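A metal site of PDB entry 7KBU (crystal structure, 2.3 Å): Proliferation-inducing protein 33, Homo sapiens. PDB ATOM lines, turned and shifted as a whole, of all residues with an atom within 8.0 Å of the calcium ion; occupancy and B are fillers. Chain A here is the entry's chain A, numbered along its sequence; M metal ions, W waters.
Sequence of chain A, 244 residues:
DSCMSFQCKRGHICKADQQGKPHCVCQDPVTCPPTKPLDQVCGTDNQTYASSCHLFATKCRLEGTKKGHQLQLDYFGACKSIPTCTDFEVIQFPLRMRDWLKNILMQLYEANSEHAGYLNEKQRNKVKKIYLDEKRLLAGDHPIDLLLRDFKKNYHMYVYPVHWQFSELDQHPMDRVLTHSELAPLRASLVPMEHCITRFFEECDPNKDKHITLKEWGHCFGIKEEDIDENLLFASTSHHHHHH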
ATOM      1  N   VAL A 177      31.649  27.326  18.059  1.00  0.00           N
ATOM      2  CA  VAL A 177      30.358  27.326  17.392  1.00  0.00           C
ATOM      3  C   VAL A 177      29.429  28.216  18.201  1.00  0.00           C
ATOM      4  O   VAL A 177      29.616  28.398  19.413  1.00  0.00           O
ATOM      5  CB  VAL A 177      29.723  25.916  17.240  1.00  0.00           C
ATOM      6  CG1 VAL A 177      30.738  24.912  16.706  1.00  0.00           C
ATOM      7  CG2 VAL A 177      29.145  25.420  18.550  1.00  0.00           C
ATOM      8  N   LEU A 178      28.442  28.795  17.511  1.00  0.00           N
ATOM      9  CA  LEU A 178      27.410  29.603  18.130  1.00  0.00           C
ATOM     10  C   LEU A 178      26.092  28.826  18.162  1.00  0.00           C
ATOM     11  O   LEU A 178      25.729  28.162  17.183  1.00  0.00           O
ATOM     12  CB  LEU A 178      27.201  30.901  17.354  1.00  0.00           C
ATOM     13  CG  LEU A 178      28.432  31.805  17.140  1.00  0.00           C
ATOM     14  CD1 LEU A 178      27.999  33.045  16.330  1.00  0.00           C
ATOM     15  CD2 LEU A 178      29.068  32.224  18.456  1.00  0.00           C
ATOM     16  N   PHE A 201      19.659  31.065  12.059  1.00  0.00           N
ATOM     17  CA  PHE A 201      19.434  29.630  11.866  1.00  0.00           C
ATOM     18  C   PHE A 201      18.551  29.341  10.661  1.00  0.00           C
ATOM     19  O   PHE A 201      18.476  28.179  10.240  1.00  0.00           O
ATOM     20  CB  PHE A 201      18.872  29.007  13.146  1.00  0.00           C
ATOM     21  CG  PHE A 201      19.880  29.019  14.265  1.00  0.00           C
ATOM     22  CD1 PHE A 201      20.867  28.064  14.335  1.00  0.00           C
ATOM     23  CD2 PHE A 201      19.899  30.054  15.186  1.00  0.00           C
ATOM     24  CE1 PHE A 201      21.834  28.095  15.330  1.00  0.00           C
ATOM     25  CE2 PHE A 201      20.860  30.113  16.171  1.00  0.00           C
ATOM     26  CZ  PHE A 201      21.833  29.124  16.243  1.00  0.00           C
ATOM     27  N   CYS A 204      22.089  31.015   8.007  1.00  0.00           N
ATOM     28  CA  CYS A 204      23.519  30.774   8.186  1.00  0.00           C
ATOM     29  C   CYS A 204      23.795  29.431   8.859  1.00  0.00           C
ATOM     30  O   CYS A 204      24.875  29.228   9.421  1.00  0.00           O
ATOM     31  CB  CYS A 204      24.136  31.946   8.963  1.00  0.00           C
ATOM     32  SG  CYS A 204      23.489  33.579   8.331  1.00  0.00           S
ATOM     33  N   ASP A 205      22.867  28.477   8.755  1.00  0.00           N
ATOM     34  CA  ASP A 205      23.044  27.129   9.288  1.00  0.00           C
ATOM     35  C   ASP A 205      22.572  26.151   8.210  1.00  0.00           C
ATOM     36  O   ASP A 205      21.550  25.476   8.361  1.00  0.00           O
ATOM     37  CB  ASP A 205      22.276  26.947  10.595  1.00  0.00           C
ATOM     38  CG  ASP A 205      22.434  25.562  11.197  1.00  0.00           C
ATOM     39  OD1 ASP A 205      23.466  24.889  10.962  1.00  0.00           O
ATOM     40  OD2 ASP A 205      21.496  25.134  11.895  1.00  0.00           O
ATOM     41  N   PRO A 206      23.317  26.042   7.109  1.00  0.00           N
ATOM     42  CA  PRO A 206      22.811  25.287   5.960  1.00  0.00           C
ATOM     43  C   PRO A 206      22.666  23.785   6.206  1.00  0.00           C
ATOM     44  O   PRO A 206      21.905  23.148   5.464  1.00  0.00           O
ATOM     45  CB  PRO A 206      23.839  25.562   4.845  1.00  0.00           C
ATOM     46  CG  PRO A 206      25.026  26.184   5.524  1.00  0.00           C
ATOM     47  CD  PRO A 206      24.532  26.824   6.776  1.00  0.00           C
ATOM     48  N   ASN A 207      23.354  23.188   7.176  1.00  0.00           N
ATOM     49  CA  ASN A 207      23.121  21.781   7.484  1.00  0.00           C
ATOM     50  C   ASN A 207      22.080  21.565   8.570  1.00  0.00           C
ATOM     51  O   ASN A 207      21.776  20.413   8.896  1.00  0.00           O
ATOM     52  CB  ASN A 207      24.439  21.063   7.837  1.00  0.00           C
ATOM     53  CG  ASN A 207      25.016  21.504   9.168  1.00  0.00           C
ATOM     54  OD1 ASN A 207      24.621  22.513   9.755  1.00  0.00           O
ATOM     55  ND2 ASN A 207      25.988  20.733   9.656  1.00  0.00           N
ATOM     56  N   LYS A 208      21.489  22.642   9.107  1.00  0.00           N
ATOM     57  CA  LYS A 208      20.333  22.598  10.015  1.00  0.00           C
ATOM     58  C   LYS A 208      20.610  21.802  11.295  1.00  0.00           C
ATOM     59  O   LYS A 208      19.700  21.220  11.881  1.00  0.00           O
ATOM     60  CB  LYS A 208      19.100  22.011   9.319  1.00  0.00           C
ATOM     61  CG  LYS A 208      18.585  22.822   8.114  1.00  0.00           C
ATOM     62  CD  LYS A 208      18.448  24.308   8.442  1.00  0.00           C
ATOM     63  CE  LYS A 208      17.911  25.138   7.273  1.00  0.00           C
ATOM     64  NZ  LYS A 208      18.304  26.594   7.369  1.00  0.00           N
ATOM     65  N   ASP A 209      21.854  21.806  11.788  1.00  0.00           N
ATOM     66  CA  ASP A 209      22.172  21.155  13.055  1.00  0.00           C
ATOM     67  C   ASP A 209      22.127  22.111  14.242  1.00  0.00           C
ATOM     68  O   ASP A 209      22.499  21.724  15.361  1.00  0.00           O
ATOM     69  CB  ASP A 209      23.539  20.447  12.976  1.00  0.00           C
ATOM     70  CG  ASP A 209      24.700  21.435  12.815  1.00  0.00           C
ATOM     71  OD1 ASP A 209      24.464  22.654  12.737  1.00  0.00           O
ATOM     72  OD2 ASP A 209      25.857  20.961  12.763  1.00  0.00           O
ATOM     73  N   LYS A 210      21.694  23.354  14.032  1.00  0.00           N
ATOM     74  CA  LYS A 210      21.458  24.323  15.112  1.00  0.00           C
ATOM     75  C   LYS A 210      22.754  24.800  15.749  1.00  0.00           C
ATOM     76  O   LYS A 210      22.728  25.384  16.843  1.00  0.00           O
ATOM     77  CB  LYS A 210      20.554  23.725  16.201  1.00  0.00           C
ATOM     78  CG  LYS A 210      19.071  23.997  16.027  1.00  0.00           C
ATOM     79  CD  LYS A 210      18.492  23.425  14.724  1.00  0.00           C
ATOM     80  CE  LYS A 210      17.563  24.453  14.044  1.00  0.00           C
ATOM     81  NZ  LYS A 210      17.106  24.005  12.687  1.00  0.00           N
ATOM     82  N   HIS A 211      23.896  24.545  15.119  1.00  0.00           N
ATOM     83  CA  HIS A 211      25.179  25.061  15.553  1.00  0.00           C
ATOM     84  C   HIS A 211      25.774  25.773  14.353  1.00  0.00           C
ATOM     85  O   HIS A 211      25.810  25.211  13.253  1.00  0.00           O
ATOM     86  CB  HIS A 211      26.116  23.961  16.048  1.00  0.00           C
ATOM     87  CG  HIS A 211      25.595  23.220  17.237  1.00  0.00           C
ATOM     88  ND1 HIS A 211      24.713  22.169  17.127  1.00  0.00           N
ATOM     89  CD2 HIS A 211      25.820  23.391  18.556  1.00  0.00           C
ATOM     90  CE1 HIS A 211      24.420  21.712  18.335  1.00  0.00           C
ATOM     91  NE2 HIS A 211      25.076  22.441  19.220  1.00  0.00           N
ATOM     92  N   ILE A 212      26.253  27.001  14.560  1.00  0.00           N
ATOM     93  CA  ILE A 212      26.832  27.811  13.491  1.00  0.00           C
ATOM     94  C   ILE A 212      28.334  27.823  13.701  1.00  0.00           C
ATOM     95  O   ILE A 212      28.824  28.355  14.704  1.00  0.00           O
ATOM     96  CB  ILE A 212      26.251  29.226  13.489  1.00  0.00           C
ATOM     97  CG1 ILE A 212      24.762  29.177  13.127  1.00  0.00           C
ATOM     98  CG2 ILE A 212      27.012  30.132  12.503  1.00  0.00           C
ATOM     99  CD1 ILE A 212      24.046  30.439  13.428  1.00  0.00           C
ATOM    100  N   THR A 213      29.052  27.231  12.757  1.00  0.00           N
ATOM    101  CA  THR A 213      30.511  27.217  12.782  1.00  0.00           C
ATOM    102  C   THR A 213      31.061  28.539  12.238  1.00  0.00           C
ATOM    103  O   THR A 213      30.338  29.348  11.637  1.00  0.00           O
ATOM    104  CB  THR A 213      31.033  26.066  11.937  1.00  0.00           C
ATOM    105  OG1 THR A 213      30.645  26.281  10.579  1.00  0.00           O
ATOM    106  CG2 THR A 213      30.470  24.741  12.428  1.00  0.00           C
ATOM    107  N   GLU A 216      30.439  28.669   8.555  1.00  0.00           N
ATOM    108  CA  GLU A 216      29.053  29.060   8.264  1.00  0.00           C
ATOM    109  C   GLU A 216      28.829  30.544   8.506  1.00  0.00           C
ATOM    110  O   GLU A 216      28.123  31.214   7.757  1.00  0.00           O
ATOM    111  CB  GLU A 216      28.081  28.217   9.102  1.00  0.00           C
ATOM    112  CG  GLU A 216      27.922  26.757   8.603  1.00  0.00           C
ATOM    113  CD  GLU A 216      27.112  25.852   9.559  1.00  0.00           C
ATOM    114  OE1 GLU A 216      27.182  26.037  10.784  1.00  0.00           O
ATOM    115  OE2 GLU A 216      26.397  24.950   9.069  1.00  0.00           O
HETATM  116 CA    CA M   1      25.532  24.209  11.300  1.00  0.00          CA
HETATM  117  O   HOH W   1      27.361  22.905  11.768  1.00  0.00           O
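Water W1 lies within hydrogen-bond range of the side-chain carboxylate of Asp 209 and the side-chain amide nitrogen of Asn 207.
The backbone NH (N) of Glu 216 is in hydrogen-bond range of the side-chain hydroxyl (OG1) of Thr 213 (3.1 Å).
The side-chain carboxylate (OD2) of Asp 205 sits at hydrogen-bond distance from the backbone NH (N) of Lys 210, at 2.8 Å.
The calcium ion is bound by OD1 of Asp 205 (2.2 Å).
O of His 211 is bound to the calcium ion (2.2 Å).
Water W1 is bound to the calcium ion, 2.3 Å away.
OD1 of Asp 209 binds the calcium ion (2.4 Å).
OD1 of Asn 207 is bound to the calcium ion, 2.5 Å away.
OE2 of Glu 216 is bound to the calcium ion (2.5 Å).
The calcium ion is bound by OE1 of Glu 216 (2.5 Å).
Five residues have an atom within 4 Å of the calcium ion: Asp 205, Asn 207, Asp 209, His 211 and Glu 216.
The nearest printed residue that does not touch the calcium ion is Ile 212 (4.4 Å).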
